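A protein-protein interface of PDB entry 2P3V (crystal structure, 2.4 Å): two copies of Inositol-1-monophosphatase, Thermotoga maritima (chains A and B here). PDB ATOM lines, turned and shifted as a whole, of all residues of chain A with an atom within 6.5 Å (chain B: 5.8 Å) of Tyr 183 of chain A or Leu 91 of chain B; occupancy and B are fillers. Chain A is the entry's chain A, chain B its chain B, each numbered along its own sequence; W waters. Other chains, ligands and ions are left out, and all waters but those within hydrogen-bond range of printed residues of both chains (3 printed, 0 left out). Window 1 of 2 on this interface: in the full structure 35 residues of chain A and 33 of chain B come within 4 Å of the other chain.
The side-chain hydroxyl (OH) of Tyr 183 of chain A lies within hydrogen-bond range of the side-chain carboxylate (OE2) of Glu 118 of chain A, at 2.5 Å. The backbone NH (N) of Val 147 of chain A sits at hydrogen-bond distance from the side-chain carboxylate (OD2) of Asp 190 of chain A (2.9 Å). N of Arg 188 of chain A lies within hydrogen-bond range of O of Tyr 183 of chain A (2.8 Å). The indole nitrogen of Trp 22 of chain B lies close to the backbone carbonyl oxygen of Gly 90 of chain B (3.2 Å). O of Asn 86 of chain B lies within hydrogen-bond range of N of Leu 91 of chain B, 2.8 Å away. The backbone carbonyl oxygen (O) of Asn 93 of chain B is in hydrogen-bond range of the side-chain amide nitrogen (ND2) of Asn 86 of chain B, 2.7 Å away.
Val 147 of chain A touches His 89 of chain B (CG2 to NE2, 3.5 Å). Arg 172 of chain A touches Leu 174 of chain B. CD2 of Leu 91 of chain B touches CD2 of Tyr 183 of chain A, 3.6 Å away. Gly 187 of chain A touches His 89 of chain B. Arg 188 of chain A touches Trp 22 of chain B. CA of Arg 188 of chain A touches O of His 89 of chain B, at 3.3 Å. Leu 91 of chain B touches Arg 188 of chain A. NH1 of Arg 188 of chain A touches CD of Pro 92 of chain B, at 3.7 Å. His 89 of chain B touches Asp 190 of chain A.
2 positions are printed for both chains. Of the 11 pairs that touch across the chains among the printed residues, none has its exchanged pair printed and touching as well.
The guanidinium group of Arg 172 of chain A sits at hydrogen-bond distance from the side-chain amide oxygen of Asn 86 of chain B, at 3.0 Å. The guanidinium group (NE) of Arg 188 of chain A sits at hydrogen-bond distance from the backbone carbonyl oxygen (O) of Gly 90 of chain B.
Of the printed residues of chain B, Val 147 of chain A touches His 89 (3.5 Å). Asn 180 of chain A touches none of the printed residues of chain B. Of the printed residues of chain B, Arg 188 of chain A touches Trp 22, His 89, Gly 90, Leu 91 and Pro 92. Of the printed residues of chain B, Asp 190 of chain A touches His 89 (3.8 Å). Of the printed residues of chain A, Leu 91 of chain B touches Tyr 183 and Arg 188. The nearest residue of chain B that does not touch Tyr 183 of chain A is Pro 92 of chain B (4.2 Å). The nearest residue of chain A that does not touch Leu 91 of chain B is Val 189 of chain A (4.1 Å).
Of the 12 printed residues of chain B, 7 touch a printed residue of chain A. Printed residues of chain B that touch a printed residue of chain A: Trp 22, Asn 86, His 89, Gly 90, Leu 91, Pro 92 and Leu 174. Hydrophobic or aromatic side chains of chain B that line the printed part of chain A: Trp 22, His 89, Leu 91 and Pro 92. Of the 24 printed residues of chain A, 6 touch a printed residue of chain B. Printed residues of chain A that touch a printed residue of chain B: Val 147, Arg 172, Tyr 183, Gly 187, Arg 188 and Asp 190. Among the printed residues, no Asp or Glu carboxylate lies within 4 Å of a Lys or Arg side-chain nitrogen of the other chain.
Water W1 lies within hydrogen-bond range of the backbone carbonyl oxygen of Gly 187 of chain A (2.7 Å), the side-chain carboxylate of Asp 190 of chain A (2.9 Å), a ring nitrogen (ND1) of His 89 of chain B (3.0 Å) and the backbone NH of Val 189 of chain A (3.2 Å). Water W3 bridges N of Asn 86 of chain B and NH1 of Arg 172 of chain A. Water W2 bridges OD1 of Asn 93 of chain A and ND2 of Asn 93 of chain B.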
ATOM      1  N   ASN A  93     -12.212   2.690  17.325  1.00  0.00           N
ATOM      2  CA  ASN A  93     -12.339   3.992  17.957  1.00  0.00           C
ATOM      3  C   ASN A  93     -13.633   4.201  18.709  1.00  0.00           C
ATOM      4  O   ASN A  93     -14.589   4.805  18.213  1.00  0.00           O
ATOM      5  CB  ASN A  93     -12.150   5.098  16.926  1.00  0.00           C
ATOM      6  CG  ASN A  93     -10.693   5.370  16.644  1.00  0.00           C
ATOM      7  OD1 ASN A  93      -9.865   4.460  16.679  1.00  0.00           O
ATOM      8  ND2 ASN A  93     -10.370   6.623  16.352  1.00  0.00           N
ATOM      9  N   ALA A 113     -10.268   3.090  25.938  1.00  0.00           N
ATOM     10  CA  ALA A 113     -10.580   2.491  24.647  1.00  0.00           C
ATOM     11  C   ALA A 113     -10.207   1.017  24.687  1.00  0.00           C
ATOM     12  O   ALA A 113      -9.067   0.647  24.406  1.00  0.00           O
ATOM     13  CB  ALA A 113      -9.804   3.194  23.541  1.00  0.00           C
ATOM     14  N   LEU A 116      -8.261  -0.557  21.905  1.00  0.00           N
ATOM     15  CA  LEU A 116      -6.937   0.007  21.661  1.00  0.00           C
ATOM     16  C   LEU A 116      -6.060  -0.064  22.897  1.00  0.00           C
ATOM     17  O   LEU A 116      -4.913   0.370  22.865  1.00  0.00           O
ATOM     18  CB  LEU A 116      -7.050   1.464  21.222  1.00  0.00           C
ATOM     19  CG  LEU A 116      -7.956   1.790  20.035  1.00  0.00           C
ATOM     20  CD1 LEU A 116      -8.211   3.283  19.982  1.00  0.00           C
ATOM     21  CD2 LEU A 116      -7.315   1.310  18.753  1.00  0.00           C
ATOM     22  N   GLU A 118      -6.095   1.698  25.407  1.00  0.00           N
ATOM     23  CA  GLU A 118      -5.669   3.055  25.718  1.00  0.00           C
ATOM     24  C   GLU A 118      -6.480   3.609  26.876  1.00  0.00           C
ATOM     25  O   GLU A 118      -7.679   3.841  26.735  1.00  0.00           O
ATOM     26  CB  GLU A 118      -5.843   3.956  24.492  1.00  0.00           C
ATOM     27  CG  GLU A 118      -4.904   3.610  23.352  1.00  0.00           C
ATOM     28  CD  GLU A 118      -5.083   4.502  22.143  1.00  0.00           C
ATOM     29  OE1 GLU A 118      -4.223   4.457  21.235  1.00  0.00           O
ATOM     30  OE2 GLU A 118      -6.084   5.239  22.094  1.00  0.00           O
ATOM     31  N   LEU A 120      -6.568   6.766  29.105  1.00  0.00           N
ATOM     32  CA  LEU A 120      -6.051   8.108  29.322  1.00  0.00           C
ATOM     33  C   LEU A 120      -6.802   8.721  30.489  1.00  0.00           C
ATOM     34  O   LEU A 120      -8.017   8.574  30.609  1.00  0.00           O
ATOM     35  CB  LEU A 120      -6.234   8.941  28.059  1.00  0.00           C
ATOM     36  CG  LEU A 120      -5.554   8.368  26.809  1.00  0.00           C
ATOM     37  CD1 LEU A 120      -6.592   7.945  25.777  1.00  0.00           C
ATOM     38  CD2 LEU A 120      -4.635   9.431  26.227  1.00  0.00           C
ATOM     39  N   PHE A 130      -1.386   8.288  30.509  1.00  0.00           N
ATOM     40  CA  PHE A 130      -1.742   7.398  29.420  1.00  0.00           C
ATOM     41  C   PHE A 130      -1.110   6.049  29.791  1.00  0.00           C
ATOM     42  O   PHE A 130       0.091   5.869  29.661  1.00  0.00           O
ATOM     43  CB  PHE A 130      -1.134   7.950  28.127  1.00  0.00           C
ATOM     44  CG  PHE A 130      -1.530   7.208  26.881  1.00  0.00           C
ATOM     45  CD1 PHE A 130      -1.271   7.767  25.631  1.00  0.00           C
ATOM     46  CD2 PHE A 130      -2.154   5.965  26.944  1.00  0.00           C
ATOM     47  CE1 PHE A 130      -1.630   7.102  24.463  1.00  0.00           C
ATOM     48  CE2 PHE A 130      -2.516   5.288  25.781  1.00  0.00           C
ATOM     49  CZ  PHE A 130      -2.255   5.859  24.538  1.00  0.00           C
ATOM     50  N   VAL A 147      -2.456  18.665  12.918  1.00  0.00           N
ATOM     51  CA  VAL A 147      -3.436  17.695  12.511  1.00  0.00           C
ATOM     52  C   VAL A 147      -4.582  17.976  13.472  1.00  0.00           C
ATOM     53  O   VAL A 147      -4.480  17.700  14.665  1.00  0.00           O
ATOM     54  CB  VAL A 147      -2.952  16.266  12.718  1.00  0.00           C
ATOM     55  CG1 VAL A 147      -4.128  15.306  12.612  1.00  0.00           C
ATOM     56  CG2 VAL A 147      -1.931  15.925  11.669  1.00  0.00           C
ATOM     57  N   ARG A 172      -8.789  14.987  10.863  1.00  0.00           N
ATOM     58  CA  ARG A 172      -9.307  13.655  11.135  1.00  0.00           C
ATOM     59  C   ARG A 172     -10.724  13.625  11.693  1.00  0.00           C
ATOM     60  O   ARG A 172     -11.157  14.546  12.385  1.00  0.00           O
ATOM     61  CB  ARG A 172      -8.394  12.942  12.140  1.00  0.00           C
ATOM     62  CG  ARG A 172      -6.965  12.750  11.691  1.00  0.00           C
ATOM     63  CD  ARG A 172      -6.878  11.750  10.555  1.00  0.00           C
ATOM     64  NE  ARG A 172      -5.537  11.708   9.977  1.00  0.00           N
ATOM     65  CZ  ARG A 172      -5.278  11.832   8.679  1.00  0.00           C
ATOM     66  NH1 ARG A 172      -4.027  11.784   8.249  1.00  0.00           N
ATOM     67  NH2 ARG A 172      -6.270  12.004   7.810  1.00  0.00           N
ATOM     68  N   LEU A 174     -12.519  10.714  13.683  1.00  0.00           N
ATOM     69  CA  LEU A 174     -12.327   9.410  14.318  1.00  0.00           C
ATOM     70  C   LEU A 174     -13.558   8.695  14.831  1.00  0.00           C
ATOM     71  O   LEU A 174     -13.595   7.461  14.850  1.00  0.00           O
ATOM     72  CB  LEU A 174     -11.325   9.557  15.461  1.00  0.00           C
ATOM     73  CG  LEU A 174     -10.017  10.247  15.080  1.00  0.00           C
ATOM     74  CD1 LEU A 174      -9.200  10.451  16.331  1.00  0.00           C
ATOM     75  CD2 LEU A 174      -9.258   9.411  14.057  1.00  0.00           C
ATOM     76  N   ALA A 178     -14.893  11.579  23.435  1.00  0.00           N
ATOM     77  CA  ALA A 178     -14.030  11.577  24.620  1.00  0.00           C
ATOM     78  C   ALA A 178     -12.579  11.262  24.273  1.00  0.00           C
ATOM     79  O   ALA A 178     -11.653  11.954  24.691  1.00  0.00           O
ATOM     80  CB  ALA A 178     -14.551  10.578  25.635  1.00  0.00           C
ATOM     81  N   LEU A 179     -12.396  10.214  23.491  1.00  0.00           N
ATOM     82  CA  LEU A 179     -11.078   9.772  23.082  1.00  0.00           C
ATOM     83  C   LEU A 179     -10.330  10.873  22.327  1.00  0.00           C
ATOM     84  O   LEU A 179      -9.177  11.188  22.630  1.00  0.00           O
ATOM     85  CB  LEU A 179     -11.244   8.540  22.195  1.00  0.00           C
ATOM     86  CG  LEU A 179     -10.014   7.795  21.709  1.00  0.00           C
ATOM     87  CD1 LEU A 179      -9.257   7.224  22.887  1.00  0.00           C
ATOM     88  CD2 LEU A 179     -10.454   6.691  20.787  1.00  0.00           C
ATOM     89  N   ASN A 180     -11.007  11.446  21.342  1.00  0.00           N
ATOM     90  CA  ASN A 180     -10.459  12.499  20.499  1.00  0.00           C
ATOM     91  C   ASN A 180      -9.975  13.651  21.375  1.00  0.00           C
ATOM     92  O   ASN A 180      -8.904  14.221  21.137  1.00  0.00           O
ATOM     93  CB  ASN A 180     -11.545  12.971  19.520  1.00  0.00           C
ATOM     94  CG  ASN A 180     -10.988  13.382  18.162  1.00  0.00           C
ATOM     95  OD1 ASN A 180     -11.681  13.287  17.140  1.00  0.00           O
ATOM     96  ND2 ASN A 180      -9.747  13.866  18.145  1.00  0.00           N
ATOM     97  N   ALA A 181     -10.756  13.990  22.397  1.00  0.00           N
ATOM     98  CA  ALA A 181     -10.377  15.076  23.298  1.00  0.00           C
ATOM     99  C   ALA A 181      -9.157  14.659  24.120  1.00  0.00           C
ATOM    100  O   ALA A 181      -8.273  15.470  24.391  1.00  0.00           O
ATOM    101  CB  ALA A 181     -11.552  15.438  24.224  1.00  0.00           C
ATOM    102  N   ALA A 182      -9.107  13.391  24.518  1.00  0.00           N
ATOM    103  CA  ALA A 182      -7.980  12.892  25.292  1.00  0.00           C
ATOM    104  C   ALA A 182      -6.733  12.895  24.405  1.00  0.00           C
ATOM    105  O   ALA A 182      -5.618  13.123  24.880  1.00  0.00           O
ATOM    106  CB  ALA A 182      -8.277  11.486  25.792  1.00  0.00           C
ATOM    107  N   TYR A 183      -6.942  12.661  23.108  1.00  0.00           N
ATOM    108  CA  TYR A 183      -5.858  12.642  22.126  1.00  0.00           C
ATOM    109  C   TYR A 183      -5.131  13.982  22.000  1.00  0.00           C
ATOM    110  O   TYR A 183      -3.934  14.028  21.695  1.00  0.00           O
ATOM    111  CB  TYR A 183      -6.406  12.209  20.777  1.00  0.00           C
ATOM    112  CG  TYR A 183      -6.416  10.712  20.595  1.00  0.00           C
ATOM    113  CD1 TYR A 183      -6.270   9.857  21.679  1.00  0.00           C
ATOM    114  CD2 TYR A 183      -6.550  10.151  19.329  1.00  0.00           C
ATOM    115  CE1 TYR A 183      -6.251   8.473  21.500  1.00  0.00           C
ATOM    116  CE2 TYR A 183      -6.536   8.778  19.142  1.00  0.00           C
ATOM    117  CZ  TYR A 183      -6.384   7.944  20.224  1.00  0.00           C
ATOM    118  OH  TYR A 183      -6.353   6.588  20.019  1.00  0.00           O
ATOM    119  N   VAL A 184      -5.861  15.071  22.213  1.00  0.00           N
ATOM    120  CA  VAL A 184      -5.261  16.393  22.178  1.00  0.00           C
ATOM    121  C   VAL A 184      -4.327  16.383  23.392  1.00  0.00           C
ATOM    122  O   VAL A 184      -3.171  16.791  23.312  1.00  0.00           O
ATOM    123  CB  VAL A 184      -6.352  17.490  22.325  1.00  0.00           C
ATOM    124  CG1 VAL A 184      -5.740  18.815  22.720  1.00  0.00           C
ATOM    125  CG2 VAL A 184      -7.084  17.658  21.014  1.00  0.00           C
ATOM    126  N   GLY A 185      -4.834  15.873  24.509  1.00  0.00           N
ATOM    127  CA  GLY A 185      -4.032  15.813  25.717  1.00  0.00           C
ATOM    128  C   GLY A 185      -2.848  14.881  25.561  1.00  0.00           C
ATOM    129  O   GLY A 185      -1.800  15.084  26.166  1.00  0.00           O
ATOM    130  N   ALA A 186      -3.014  13.836  24.761  1.00  0.00           N
ATOM    131  CA  ALA A 186      -1.921  12.903  24.536  1.00  0.00           C
ATOM    132  C   ALA A 186      -0.930  13.544  23.562  1.00  0.00           C
ATOM    133  O   ALA A 186       0.245  13.167  23.527  1.00  0.00           O
ATOM    134  CB  ALA A 186      -2.451  11.596  23.963  1.00  0.00           C
ATOM    135  N   GLY A 187      -1.413  14.512  22.780  1.00  0.00           N
ATOM    136  CA  GLY A 187      -0.574  15.192  21.805  1.00  0.00           C
ATOM    137  C   GLY A 187      -0.604  14.556  20.419  1.00  0.00           C
ATOM    138  O   GLY A 187       0.259  14.846  19.580  1.00  0.00           O
ATOM    139  N   ARG A 188      -1.602  13.703  20.171  1.00  0.00           N
ATOM    140  CA  ARG A 188      -1.750  13.001  18.892  1.00  0.00           C
ATOM    141  C   ARG A 188      -2.411  13.864  17.820  1.00  0.00           C
ATOM    142  O   ARG A 188      -2.342  13.556  16.625  1.00  0.00           O
ATOM    143  CB  ARG A 188      -2.544  11.709  19.102  1.00  0.00           C
ATOM    144  CG  ARG A 188      -1.843  10.751  20.063  1.00  0.00           C
ATOM    145  CD  ARG A 188      -2.658   9.504  20.311  1.00  0.00           C
ATOM    146  NE  ARG A 188      -1.803   8.387  20.696  1.00  0.00           N
ATOM    147  CZ  ARG A 188      -2.214   7.124  20.743  1.00  0.00           C
ATOM    148  NH1 ARG A 188      -3.470   6.821  20.440  1.00  0.00           N
ATOM    149  NH2 ARG A 188      -1.366   6.158  21.051  1.00  0.00           N
ATOM    150  N   VAL A 189      -3.073  14.927  18.262  1.00  0.00           N
ATOM    151  CA  VAL A 189      -3.708  15.899  17.375  1.00  0.00           C
ATOM    152  C   VAL A 189      -3.495  17.223  18.095  1.00  0.00           C
ATOM    153  O   VAL A 189      -3.285  17.242  19.312  1.00  0.00           O
ATOM    154  CB  VAL A 189      -5.211  15.631  17.153  1.00  0.00           C
ATOM    155  CG1 VAL A 189      -5.385  14.410  16.249  1.00  0.00           C
ATOM    156  CG2 VAL A 189      -5.916  15.435  18.485  1.00  0.00           C
ATOM    157  N   ASP A 190      -3.534  18.328  17.361  1.00  0.00           N
ATOM    158  CA  ASP A 190      -3.259  19.613  17.984  1.00  0.00           C
ATOM    159  C   ASP A 190      -4.511  20.367  18.396  1.00  0.00           C
ATOM    160  O   ASP A 190      -4.446  21.329  19.161  1.00  0.00           O
ATOM    161  CB  ASP A 190      -2.379  20.443  17.040  1.00  0.00           C
ATOM    162  CG  ASP A 190      -1.166  19.656  16.528  1.00  0.00           C
ATOM    163  OD1 ASP A 190      -0.344  19.211  17.353  1.00  0.00           O
ATOM    164  OD2 ASP A 190      -1.027  19.481  15.302  1.00  0.00           O
ATOM    165  N   ILE A 208      -8.524  16.106  31.250  1.00  0.00           N
ATOM    166  CA  ILE A 208      -7.352  15.439  30.703  1.00  0.00           C
ATOM    167  C   ILE A 208      -6.581  16.472  29.880  1.00  0.00           C
ATOM    168  O   ILE A 208      -5.377  16.638  30.061  1.00  0.00           O
ATOM    169  CB  ILE A 208      -7.736  14.224  29.818  1.00  0.00           C
ATOM    170  CG1 ILE A 208      -8.276  13.098  30.691  1.00  0.00           C
ATOM    171  CG2 ILE A 208      -6.517  13.706  29.072  1.00  0.00           C
ATOM    172  CD1 ILE A 208      -8.824  11.940  29.909  1.00  0.00           C
ATOM    173  N   VAL A 209      -7.276  17.195  29.004  1.00  0.00           N
ATOM    174  CA  VAL A 209      -6.612  18.208  28.186  1.00  0.00           C
ATOM    175  C   VAL A 209      -6.013  19.313  29.054  1.00  0.00           C
ATOM    176  O   VAL A 209      -4.883  19.729  28.829  1.00  0.00           O
ATOM    177  CB  VAL A 209      -7.584  18.820  27.157  1.00  0.00           C
ATOM    178  CG1 VAL A 209      -6.904  19.953  26.398  1.00  0.00           C
ATOM    179  CG2 VAL A 209      -8.044  17.747  26.185  1.00  0.00           C
ATOM    180  N   TRP B  22       7.459   5.456  16.384  1.00  0.00           N
ATOM    181  CA  TRP B  22       6.081   5.956  16.359  1.00  0.00           C
ATOM    182  C   TRP B  22       5.849   7.147  17.292  1.00  0.00           C
ATOM    183  O   TRP B  22       5.971   7.013  18.505  1.00  0.00           O
ATOM    184  CB  TRP B  22       5.132   4.810  16.725  1.00  0.00           C
ATOM    185  CG  TRP B  22       3.685   5.168  16.750  1.00  0.00           C
ATOM    186  CD1 TRP B  22       3.038   6.043  15.922  1.00  0.00           C
ATOM    187  CD2 TRP B  22       2.681   4.614  17.607  1.00  0.00           C
ATOM    188  NE1 TRP B  22       1.692   6.065  16.212  1.00  0.00           N
ATOM    189  CE2 TRP B  22       1.448   5.196  17.241  1.00  0.00           C
ATOM    190  CE3 TRP B  22       2.702   3.681  18.647  1.00  0.00           C
ATOM    191  CZ2 TRP B  22       0.251   4.872  17.882  1.00  0.00           C
ATOM    192  CZ3 TRP B  22       1.505   3.361  19.282  1.00  0.00           C
ATOM    193  CH2 TRP B  22       0.303   3.955  18.897  1.00  0.00           C
ATOM    194  N   ASN B  86       0.050  10.366  10.365  1.00  0.00           N
ATOM    195  CA  ASN B  86      -0.503   9.822  11.602  1.00  0.00           C
ATOM    196  C   ASN B  86       0.654   9.264  12.417  1.00  0.00           C
ATOM    197  O   ASN B  86       0.756   9.490  13.630  1.00  0.00           O
ATOM    198  CB  ASN B  86      -1.490   8.691  11.316  1.00  0.00           C
ATOM    199  CG  ASN B  86      -2.867   9.197  10.982  1.00  0.00           C
ATOM    200  OD1 ASN B  86      -3.194  10.339  11.268  1.00  0.00           O
ATOM    201  ND2 ASN B  86      -3.690   8.345  10.396  1.00  0.00           N
ATOM    202  N   PHE B  87       1.516   8.528  11.720  1.00  0.00           N
ATOM    203  CA  PHE B  87       2.697   7.910  12.307  1.00  0.00           C
ATOM    204  C   PHE B  87       3.522   8.936  13.083  1.00  0.00           C
ATOM    205  O   PHE B  87       3.919   8.693  14.219  1.00  0.00           O
ATOM    206  CB  PHE B  87       3.556   7.267  11.202  1.00  0.00           C
ATOM    207  CG  PHE B  87       4.796   6.585  11.713  1.00  0.00           C
ATOM    208  CD1 PHE B  87       6.008   7.261  11.765  1.00  0.00           C
ATOM    209  CD2 PHE B  87       4.735   5.289  12.206  1.00  0.00           C
ATOM    210  CE1 PHE B  87       7.146   6.660  12.303  1.00  0.00           C
ATOM    211  CE2 PHE B  87       5.870   4.673  12.750  1.00  0.00           C
ATOM    212  CZ  PHE B  87       7.074   5.363  12.799  1.00  0.00           C
ATOM    213  N   VAL B  88       3.769  10.086  12.467  1.00  0.00           N
ATOM    214  CA  VAL B  88       4.554  11.140  13.098  1.00  0.00           C
ATOM    215  C   VAL B  88       3.860  11.765  14.302  1.00  0.00           C
ATOM    216  O   VAL B  88       4.507  12.080  15.298  1.00  0.00           O
ATOM    217  CB  VAL B  88       4.878  12.256  12.079  1.00  0.00           C
ATOM    218  CG1 VAL B  88       5.442  13.485  12.790  1.00  0.00           C
ATOM    219  CG2 VAL B  88       5.868  11.737  11.061  1.00  0.00           C
ATOM    220  N   HIS B  89       2.546  11.948  14.206  1.00  0.00           N
ATOM    221  CA  HIS B  89       1.777  12.558  15.283  1.00  0.00           C
ATOM    222  C   HIS B  89       1.481  11.600  16.407  1.00  0.00           C
ATOM    223  O   HIS B  89       1.087  12.013  17.500  1.00  0.00           O
ATOM    224  CB  HIS B  89       0.489  13.160  14.722  1.00  0.00           C
ATOM    225  CG  HIS B  89       0.718  14.441  13.997  1.00  0.00           C
ATOM    226  ND1 HIS B  89       0.490  15.670  14.576  1.00  0.00           N
ATOM    227  CD2 HIS B  89       1.295  14.692  12.797  1.00  0.00           C
ATOM    228  CE1 HIS B  89       0.924  16.622  13.767  1.00  0.00           C
ATOM    229  NE2 HIS B  89       1.418  16.053  12.681  1.00  0.00           N
ATOM    230  N   GLY B  90       1.685  10.317  16.140  1.00  0.00           N
ATOM    231  CA  GLY B  90       1.451   9.326  17.167  1.00  0.00           C
ATOM    232  C   GLY B  90       0.107   8.640  17.091  1.00  0.00           C
ATOM    233  O   GLY B  90      -0.253   7.908  18.009  1.00  0.00           O
ATOM    234  N   LEU B  91      -0.643   8.871  16.017  1.00  0.00           N
ATOM    235  CA  LEU B  91      -1.940   8.226  15.880  1.00  0.00           C
ATOM    236  C   LEU B  91      -1.695   6.791  15.479  1.00  0.00           C
ATOM    237  O   LEU B  91      -0.735   6.497  14.775  1.00  0.00           O
ATOM    238  CB  LEU B  91      -2.782   8.941  14.841  1.00  0.00           C
ATOM    239  CG  LEU B  91      -3.300  10.269  15.391  1.00  0.00           C
ATOM    240  CD1 LEU B  91      -3.823  11.122  14.266  1.00  0.00           C
ATOM    241  CD2 LEU B  91      -4.384  10.000  16.432  1.00  0.00           C
ATOM    242  N   PRO B  92      -2.560   5.871  15.926  1.00  0.00           N
ATOM    243  CA  PRO B  92      -2.387   4.457  15.597  1.00  0.00           C
ATOM    244  C   PRO B  92      -2.756   4.028  14.176  1.00  0.00           C
ATOM    245  O   PRO B  92      -2.361   2.950  13.729  1.00  0.00           O
ATOM    246  CB  PRO B  92      -3.214   3.764  16.675  1.00  0.00           C
ATOM    247  CG  PRO B  92      -4.367   4.709  16.836  1.00  0.00           C
ATOM    248  CD  PRO B  92      -3.713   6.072  16.825  1.00  0.00           C
ATOM    249  N   ASN B  93      -3.496   4.867  13.460  1.00  0.00           N
ATOM    250  CA  ASN B  93      -3.899   4.534  12.094  1.00  0.00           C
ATOM    251  C   ASN B  93      -2.832   4.777  11.042  1.00  0.00           C
ATOM    252  O   ASN B  93      -2.770   5.848  10.444  1.00  0.00           O
ATOM    253  CB  ASN B  93      -5.166   5.297  11.697  1.00  0.00           C
ATOM    254  CG  ASN B  93      -6.398   4.749  12.361  1.00  0.00           C
ATOM    255  OD1 ASN B  93      -6.965   3.763  11.909  1.00  0.00           O
ATOM    256  ND2 ASN B  93      -6.808   5.372  13.457  1.00  0.00           N
ATOM    257  N   PHE B  94      -1.991   3.769  10.846  1.00  0.00           N
ATOM    258  CA  PHE B  94      -0.932   3.778   9.848  1.00  0.00           C
ATOM    259  C   PHE B  94      -0.604   2.311   9.634  1.00  0.00           C
ATOM    260  O   PHE B  94      -0.733   1.504  10.556  1.00  0.00           O
ATOM    261  CB  PHE B  94       0.301   4.575  10.324  1.00  0.00           C
ATOM    262  CG  PHE B  94       1.054   3.953  11.478  1.00  0.00           C
ATOM    263  CD1 PHE B  94       2.016   2.961  11.259  1.00  0.00           C
ATOM    264  CD2 PHE B  94       0.821   4.382  12.787  1.00  0.00           C
ATOM    265  CE1 PHE B  94       2.737   2.414  12.320  1.00  0.00           C
ATOM    266  CE2 PHE B  94       1.540   3.836  13.858  1.00  0.00           C
ATOM    267  CZ  PHE B  94       2.497   2.850  13.619  1.00  0.00           C
ATOM    268  N   ALA B 115       0.608  -0.559  15.475  1.00  0.00           N
ATOM    269  CA  ALA B 115      -0.001   0.002  16.668  1.00  0.00           C
ATOM    270  C   ALA B 115      -1.273  -0.717  17.071  1.00  0.00           C
ATOM    271  O   ALA B 115      -1.558  -0.869  18.257  1.00  0.00           O
ATOM    272  CB  ALA B 115      -0.284   1.483  16.462  1.00  0.00           C
ATOM    273  N   LEU B 174      -9.792   8.354   8.796  1.00  0.00           N
ATOM    274  CA  LEU B 174      -8.813   7.766   9.696  1.00  0.00           C
ATOM    275  C   LEU B 174      -7.345   8.056   9.392  1.00  0.00           C
ATOM    276  O   LEU B 174      -6.559   8.309  10.313  1.00  0.00           O
ATOM    277  CB  LEU B 174      -9.046   6.265   9.739  1.00  0.00           C
ATOM    278  CG  LEU B 174     -10.523   5.967   9.978  1.00  0.00           C
ATOM    279  CD1 LEU B 174     -10.817   4.499   9.714  1.00  0.00           C
ATOM    280  CD2 LEU B 174     -10.877   6.368  11.398  1.00  0.00           C
HETATM  281  O   HOH W   1      -0.292  16.326  17.415  1.00  0.00           O
HETATM  282  O   HOH W   2      -7.831   3.002  15.320  1.00  0.00           O
HETATM  283  O   HOH W   3      -1.771   9.918   8.373  1.00  0.00           O
